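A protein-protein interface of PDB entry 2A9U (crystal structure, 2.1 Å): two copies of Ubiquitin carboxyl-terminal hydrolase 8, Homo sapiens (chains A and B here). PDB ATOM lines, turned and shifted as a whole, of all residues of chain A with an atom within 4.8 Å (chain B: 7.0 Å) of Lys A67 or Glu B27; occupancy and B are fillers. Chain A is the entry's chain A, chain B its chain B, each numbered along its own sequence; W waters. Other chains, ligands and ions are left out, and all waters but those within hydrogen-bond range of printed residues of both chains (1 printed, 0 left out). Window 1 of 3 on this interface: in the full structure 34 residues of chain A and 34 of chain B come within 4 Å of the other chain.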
ATOM      1  N   ILE A  45     -22.082 -35.892   0.399  1.00  0.00           N
ATOM      2  CA  ILE A  45     -22.945 -35.179   1.371  1.00  0.00           C
ATOM      3  C   ILE A  45     -24.338 -34.959   0.764  1.00  0.00           C
ATOM      4  O   ILE A  45     -25.342 -35.216   1.405  1.00  0.00           O
ATOM      5  CB  ILE A  45     -22.307 -33.845   1.834  1.00  0.00           C
ATOM      6  CG1 ILE A  45     -21.085 -34.109   2.725  1.00  0.00           C
ATOM      7  CG2 ILE A  45     -23.285 -32.998   2.660  1.00  0.00           C
ATOM      8  CD1 ILE A  45     -20.049 -32.949   2.673  1.00  0.00           C
ATOM      9  N   VAL A  63     -28.685 -30.549   8.295  1.00  0.00           N
ATOM     10  CA  VAL A  63     -27.231 -30.487   8.554  1.00  0.00           C
ATOM     11  C   VAL A  63     -26.392 -30.757   7.274  1.00  0.00           C
ATOM     12  O   VAL A  63     -25.407 -30.100   7.009  1.00  0.00           O
ATOM     13  CB  VAL A  63     -26.850 -31.451   9.684  1.00  0.00           C
ATOM     14  CG1 VAL A  63     -25.343 -31.863   9.642  1.00  0.00           C
ATOM     15  CG2 VAL A  63     -27.244 -30.833  11.056  1.00  0.00           C
ATOM     16  N   LEU A  64     -26.818 -31.730   6.495  1.00  0.00           N
ATOM     17  CA  LEU A  64     -26.108 -32.146   5.305  1.00  0.00           C
ATOM     18  C   LEU A  64     -26.301 -31.140   4.189  1.00  0.00           C
ATOM     19  O   LEU A  64     -25.330 -30.767   3.548  1.00  0.00           O
ATOM     20  CB  LEU A  64     -26.548 -33.561   4.918  1.00  0.00           C
ATOM     21  CG  LEU A  64     -26.138 -34.600   5.962  1.00  0.00           C
ATOM     22  CD1 LEU A  64     -26.949 -35.913   5.856  1.00  0.00           C
ATOM     23  CD2 LEU A  64     -24.624 -34.882   5.948  1.00  0.00           C
ATOM     24  N   TYR A  65     -27.515 -30.625   3.984  1.00  0.00           N
ATOM     25  CA  TYR A  65     -27.687 -29.553   2.972  1.00  0.00           C
ATOM     26  C   TYR A  65     -26.888 -28.296   3.278  1.00  0.00           C
ATOM     27  O   TYR A  65     -26.377 -27.647   2.368  1.00  0.00           O
ATOM     28  CB  TYR A  65     -29.143 -29.163   2.737  1.00  0.00           C
ATOM     29  CG  TYR A  65     -29.949 -30.183   1.965  1.00  0.00           C
ATOM     30  CD1 TYR A  65     -29.583 -30.581   0.647  1.00  0.00           C
ATOM     31  CD2 TYR A  65     -31.106 -30.738   2.529  1.00  0.00           C
ATOM     32  CE1 TYR A  65     -30.348 -31.514  -0.077  1.00  0.00           C
ATOM     33  CE2 TYR A  65     -31.876 -31.681   1.813  1.00  0.00           C
ATOM     34  CZ  TYR A  65     -31.491 -32.059   0.523  1.00  0.00           C
ATOM     35  OH  TYR A  65     -32.270 -32.969  -0.122  1.00  0.00           O
ATOM     36  N   MET A  66     -26.795 -27.945   4.555  1.00  0.00           N
ATOM     37  CA  MET A  66     -26.029 -26.778   5.023  1.00  0.00           C
ATOM     38  C   MET A  66     -24.507 -27.016   4.909  1.00  0.00           C
ATOM     39  O   MET A  66     -23.742 -26.113   4.557  1.00  0.00           O
ATOM     40  CB  MET A  66     -26.424 -26.538   6.478  1.00  0.00           C
ATOM     41  CG  MET A  66     -26.204 -25.134   7.036  1.00  0.00           C
ATOM     42  SD  MET A  66     -26.885 -23.661   5.921  1.00  0.00           S
ATOM     43  CE  MET A  66     -28.734 -23.726   6.338  1.00  0.00           C
ATOM     44  N   LYS A  67     -24.074 -28.227   5.243  1.00  0.00           N
ATOM     45  CA  LYS A  67     -22.669 -28.605   5.145  1.00  0.00           C
ATOM     46  C   LYS A  67     -22.228 -28.589   3.662  1.00  0.00           C
ATOM     47  O   LYS A  67     -21.124 -28.162   3.333  1.00  0.00           O
ATOM     48  CB  LYS A  67     -22.443 -29.984   5.781  1.00  0.00           C
ATOM     49  CG  LYS A  67     -20.943 -30.365   5.923  1.00  0.00           C
ATOM     50  CD  LYS A  67     -20.793 -31.681   6.720  1.00  0.00           C
ATOM     51  CE  LYS A  67     -19.361 -32.139   6.763  1.00  0.00           C
ATOM     52  NZ  LYS A  67     -18.665 -31.768   8.030  1.00  0.00           N
ATOM     53  N   TYR A  68     -23.113 -29.027   2.775  1.00  0.00           N
ATOM     54  CA  TYR A  68     -22.877 -29.002   1.314  1.00  0.00           C
ATOM     55  C   TYR A  68     -22.673 -27.561   0.851  1.00  0.00           C
ATOM     56  O   TYR A  68     -21.716 -27.267   0.103  1.00  0.00           O
ATOM     57  CB  TYR A  68     -24.052 -29.658   0.560  1.00  0.00           C
ATOM     58  CG  TYR A  68     -23.956 -29.642  -0.963  1.00  0.00           C
ATOM     59  CD1 TYR A  68     -23.376 -30.713  -1.661  1.00  0.00           C
ATOM     60  CD2 TYR A  68     -24.444 -28.550  -1.711  1.00  0.00           C
ATOM     61  CE1 TYR A  68     -23.303 -30.703  -3.067  1.00  0.00           C
ATOM     62  CE2 TYR A  68     -24.377 -28.531  -3.087  1.00  0.00           C
ATOM     63  CZ  TYR A  68     -23.800 -29.615  -3.761  1.00  0.00           C
ATOM     64  OH  TYR A  68     -23.753 -29.605  -5.119  1.00  0.00           O
ATOM     65  N   VAL A  69     -23.553 -26.661   1.304  1.00  0.00           N
ATOM     66  CA  VAL A  69     -23.455 -25.231   0.939  1.00  0.00           C
ATOM     67  C   VAL A  69     -22.160 -24.633   1.522  1.00  0.00           C
ATOM     68  O   VAL A  69     -21.473 -23.875   0.863  1.00  0.00           O
ATOM     69  CB  VAL A  69     -24.709 -24.412   1.395  1.00  0.00           C
ATOM     70  CG1 VAL A  69     -24.521 -22.945   1.098  1.00  0.00           C
ATOM     71  CG2 VAL A  69     -26.007 -24.929   0.708  1.00  0.00           C
ATOM     72  N   THR A  70     -21.831 -24.997   2.761  1.00  0.00           N
ATOM     73  CA  THR A  70     -20.576 -24.584   3.391  1.00  0.00           C
ATOM     74  C   THR A  70     -19.355 -25.035   2.560  1.00  0.00           C
ATOM     75  O   THR A  70     -18.441 -24.252   2.304  1.00  0.00           O
ATOM     76  CB  THR A  70     -20.540 -25.058   4.872  1.00  0.00           C
ATOM     77  OG1 THR A  70     -21.712 -24.522   5.560  1.00  0.00           O
ATOM     78  CG2 THR A  70     -19.282 -24.586   5.587  1.00  0.00           C
ATOM     79  N   VAL A  71     -19.346 -26.278   2.106  1.00  0.00           N
ATOM     80  CA  VAL A  71     -18.222 -26.797   1.300  1.00  0.00           C
ATOM     81  C   VAL A  71     -18.075 -25.977   0.001  1.00  0.00           C
ATOM     82  O   VAL A  71     -16.964 -25.579  -0.407  1.00  0.00           O
ATOM     83  CB  VAL A  71     -18.423 -28.278   1.009  1.00  0.00           C
ATOM     84  CG1 VAL A  71     -17.566 -28.738  -0.178  1.00  0.00           C
ATOM     85  CG2 VAL A  71     -18.093 -29.105   2.260  1.00  0.00           C
ATOM     86  N   LEU B  22     -27.352 -27.662  16.025  1.00  0.00           N
ATOM     87  CA  LEU B  22     -27.371 -28.231  14.682  1.00  0.00           C
ATOM     88  C   LEU B  22     -26.355 -27.523  13.764  1.00  0.00           C
ATOM     89  O   LEU B  22     -25.617 -28.204  13.011  1.00  0.00           O
ATOM     90  CB  LEU B  22     -28.780 -28.084  14.138  1.00  0.00           C
ATOM     91  CG  LEU B  22     -29.429 -29.310  13.548  1.00  0.00           C
ATOM     92  CD1 LEU B  22     -29.195 -30.532  14.433  1.00  0.00           C
ATOM     93  CD2 LEU B  22     -30.898 -29.063  13.290  1.00  0.00           C
ATOM     94  N   ASN B  23     -26.279 -26.180  13.866  1.00  0.00           N
ATOM     95  CA  ASN B  23     -25.376 -25.357  13.038  1.00  0.00           C
ATOM     96  C   ASN B  23     -23.894 -25.658  13.234  1.00  0.00           C
ATOM     97  O   ASN B  23     -23.117 -25.653  12.278  1.00  0.00           O
ATOM     98  CB  ASN B  23     -25.661 -23.871  13.223  1.00  0.00           C
ATOM     99  CG  ASN B  23     -26.834 -23.386  12.365  1.00  0.00           C
ATOM    100  OD1 ASN B  23     -27.287 -24.076  11.466  1.00  0.00           O
ATOM    101  ND2 ASN B  23     -27.304 -22.178  12.630  1.00  0.00           N
ATOM    102  N   LYS B  24     -23.522 -26.001  14.464  1.00  0.00           N
ATOM    103  CA  LYS B  24     -22.173 -26.518  14.767  1.00  0.00           C
ATOM    104  C   LYS B  24     -21.768 -27.729  13.895  1.00  0.00           C
ATOM    105  O   LYS B  24     -20.607 -27.874  13.544  1.00  0.00           O
ATOM    106  CB  LYS B  24     -22.091 -26.887  16.252  1.00  0.00           C
ATOM    107  CG  LYS B  24     -22.414 -25.705  17.155  1.00  0.00           C
ATOM    108  CD  LYS B  24     -22.437 -26.128  18.629  1.00  0.00           C
ATOM    109  CE  LYS B  24     -22.757 -24.944  19.555  1.00  0.00           C
ATOM    110  NZ  LYS B  24     -23.264 -25.434  20.883  1.00  0.00           N
ATOM    111  N   LYS B  25     -22.733 -28.564  13.525  1.00  0.00           N
ATOM    112  CA  LYS B  25     -22.469 -29.773  12.763  1.00  0.00           C
ATOM    113  C   LYS B  25     -22.242 -29.503  11.290  1.00  0.00           C
ATOM    114  O   LYS B  25     -21.856 -30.408  10.563  1.00  0.00           O
ATOM    115  CB  LYS B  25     -23.660 -30.727  12.908  1.00  0.00           C
ATOM    116  CG  LYS B  25     -23.863 -31.233  14.347  1.00  0.00           C
ATOM    117  CD  LYS B  25     -25.191 -31.937  14.465  1.00  0.00           C
ATOM    118  CE  LYS B  25     -25.060 -33.190  15.333  1.00  0.00           C
ATOM    119  NZ  LYS B  25     -25.149 -32.919  16.796  1.00  0.00           N
ATOM    120  N   THR B  26     -22.513 -28.266  10.862  1.00  0.00           N
ATOM    121  CA  THR B  26     -22.454 -27.916   9.451  1.00  0.00           C
ATOM    122  C   THR B  26     -21.098 -27.377   9.028  1.00  0.00           C
ATOM    123  O   THR B  26     -20.874 -27.149   7.845  1.00  0.00           O
ATOM    124  CB  THR B  26     -23.522 -26.893   9.064  1.00  0.00           C
ATOM    125  OG1 THR B  26     -23.198 -25.606   9.613  1.00  0.00           O
ATOM    126  CG2 THR B  26     -24.939 -27.345   9.524  1.00  0.00           C
ATOM    127  N   GLU B  27     -20.212 -27.171  10.002  1.00  0.00           N
ATOM    128  CA  GLU B  27     -18.971 -26.436   9.783  1.00  0.00           C
ATOM    129  C   GLU B  27     -17.913 -27.376   9.226  1.00  0.00           C
ATOM    130  O   GLU B  27     -17.928 -28.546   9.531  1.00  0.00           O
ATOM    131  CB  GLU B  27     -18.464 -25.798  11.079  1.00  0.00           C
ATOM    132  CG  GLU B  27     -19.407 -24.742  11.680  1.00  0.00           C
ATOM    133  CD  GLU B  27     -19.565 -23.489  10.821  1.00  0.00           C
ATOM    134  OE1 GLU B  27     -18.801 -23.273   9.830  1.00  0.00           O
ATOM    135  OE2 GLU B  27     -20.499 -22.716  11.135  1.00  0.00           O
ATOM    136  N   VAL B  28     -17.019 -26.839   8.402  1.00  0.00           N
ATOM    137  CA  VAL B  28     -15.900 -27.596   7.848  1.00  0.00           C
ATOM    138  C   VAL B  28     -14.554 -26.919   8.177  1.00  0.00           C
ATOM    139  O   VAL B  28     -13.491 -27.548   8.086  1.00  0.00           O
ATOM    140  CB  VAL B  28     -16.058 -27.886   6.276  1.00  0.00           C
ATOM    141  CG1 VAL B  28     -17.450 -28.471   5.942  1.00  0.00           C
ATOM    142  CG2 VAL B  28     -15.797 -26.678   5.453  1.00  0.00           C
ATOM    143  N   LYS B  29     -14.584 -25.657   8.586  1.00  0.00           N
ATOM    144  CA  LYS B  29     -13.322 -25.002   8.959  1.00  0.00           C
ATOM    145  C   LYS B  29     -13.000 -25.253  10.421  1.00  0.00           C
ATOM    146  O   LYS B  29     -13.851 -25.010  11.286  1.00  0.00           O
ATOM    147  CB  LYS B  29     -13.406 -23.499   8.723  1.00  0.00           C
ATOM    148  CG  LYS B  29     -13.441 -23.117   7.259  1.00  0.00           C
ATOM    149  CD  LYS B  29     -13.419 -21.618   7.093  1.00  0.00           C
ATOM    150  CE  LYS B  29     -13.188 -21.298   5.617  1.00  0.00           C
ATOM    151  NZ  LYS B  29     -13.499 -19.892   5.246  1.00  0.00           N
ATOM    152  N   PRO B  30     -11.770 -25.720  10.714  1.00  0.00           N
ATOM    153  CA  PRO B  30     -11.317 -25.946  12.112  1.00  0.00           C
ATOM    154  C   PRO B  30     -11.492 -24.709  12.981  1.00  0.00           C
ATOM    155  O   PRO B  30     -11.783 -24.814  14.173  1.00  0.00           O
ATOM    156  CB  PRO B  30      -9.835 -26.271  11.926  1.00  0.00           C
ATOM    157  CG  PRO B  30      -9.855 -27.049  10.555  1.00  0.00           C
ATOM    158  CD  PRO B  30     -10.730 -26.130   9.741  1.00  0.00           C
ATOM    159  N   LYS B  32     -13.768 -22.813  13.053  1.00  0.00           N
ATOM    160  CA  LYS B  32     -15.174 -22.616  13.433  1.00  0.00           C
ATOM    161  C   LYS B  32     -15.723 -23.883  14.093  1.00  0.00           C
ATOM    162  O   LYS B  32     -16.936 -24.031  14.217  1.00  0.00           O
ATOM    163  CB  LYS B  32     -16.019 -22.218  12.232  1.00  0.00           C
ATOM    164  CG  LYS B  32     -15.421 -21.068  11.380  1.00  0.00           C
ATOM    165  CD  LYS B  32     -16.382 -20.568  10.338  1.00  0.00           C
ATOM    166  CE  LYS B  32     -17.350 -19.610  10.967  1.00  0.00           C
ATOM    167  NZ  LYS B  32     -18.279 -19.079   9.928  1.00  0.00           N
ATOM    168  N   ILE B  33     -14.810 -24.783  14.488  1.00  0.00           N
ATOM    169  CA  ILE B  33     -15.123 -26.007  15.233  1.00  0.00           C
ATOM    170  C   ILE B  33     -14.400 -26.035  16.584  1.00  0.00           C
ATOM    171  O   ILE B  33     -13.160 -26.158  16.692  1.00  0.00           O
ATOM    172  CB  ILE B  33     -14.816 -27.327  14.426  1.00  0.00           C
ATOM    173  CG1 ILE B  33     -15.602 -27.371  13.090  1.00  0.00           C
ATOM    174  CG2 ILE B  33     -15.179 -28.539  15.281  1.00  0.00           C
ATOM    175  CD1 ILE B  33     -14.919 -28.186  11.917  1.00  0.00           C
HETATM  176  O   HOH W   1     -21.992 -23.803   8.173  1.00  0.00           O
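The backbone carbonyl oxygen (O) of Met A66 sits at hydrogen-bond distance from the side-chain hydroxyl (OG1) of Thr A70 (2.8 Å). The backbone carbonyl oxygen of Asn B23 is in hydrogen-bond range of the side-chain hydroxyl of Thr B26 (2.7 Å).
CG of Leu B22 touches CG2 of Val A63, at 3.6 Å. Lys B25 touches Val A63. Val A63 touches Thr B26. CG2 of Thr B26 touches CB of Met A66, 3.5 Å away. Thr B26 touches Lys A67. O of Glu B27 touches NZ of Lys A67 (3.6 Å). Lys A67 touches Val B28. Thr A70 touches Thr B26 (OG1 to O, 3.6 Å). Val B28 touches Val A71.
Printed residues of chain B within 4 Å of Val A63: Leu B22 (3.6 Å), Lys B25 (3.8 Å) and Thr B26 (3.8 Å). Printed residues of chain B within 4 Å of Met A66: Thr B26. Lys A67 touches three residues of chain B. Tyr A68 touches none of the printed residues of chain B. Of the printed residues of chain B, Thr A70 touches Thr B26. Of the printed residues of chain B, Val A71 touches Val B28. Of chain A, only Lys A67 (3.6 Å) comes within 4 Å of Glu B27. Printed residues of chain A within 4 Å of Val B28: Lys A67 (3.97 Å) and Val A71 (3.8 Å). The nearest residue of chain B that does not touch Lys A67 is Lys B25 (4.2 Å). The nearest printed residue of chain A that does not touch Lys B25 is Lys A67 (4.2 Å).
Printed residues of chain A that touch a printed residue of chain B: Val A63, Met A66, Lys A67, Thr A70 and Val A71. Hydrophobic or aromatic side chains of chain A within 4 Å of the printed part of chain B: Val A63, Met A66 and Val A71. Among the printed residues, 9 pairs touch across the chains.
No position is printed for both chains. Of the 9 pairs that touch across the chains among the printed residues, none has its exchanged pair printed and touching as well.
Water W1 lies within hydrogen-bond range of the side-chain hydroxyl of Thr B26 (2.6 Å), the side-chain hydroxyl of Thr A70 (2.7 Å) and the side-chain carboxylate of Glu B27 (3.5 Å).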
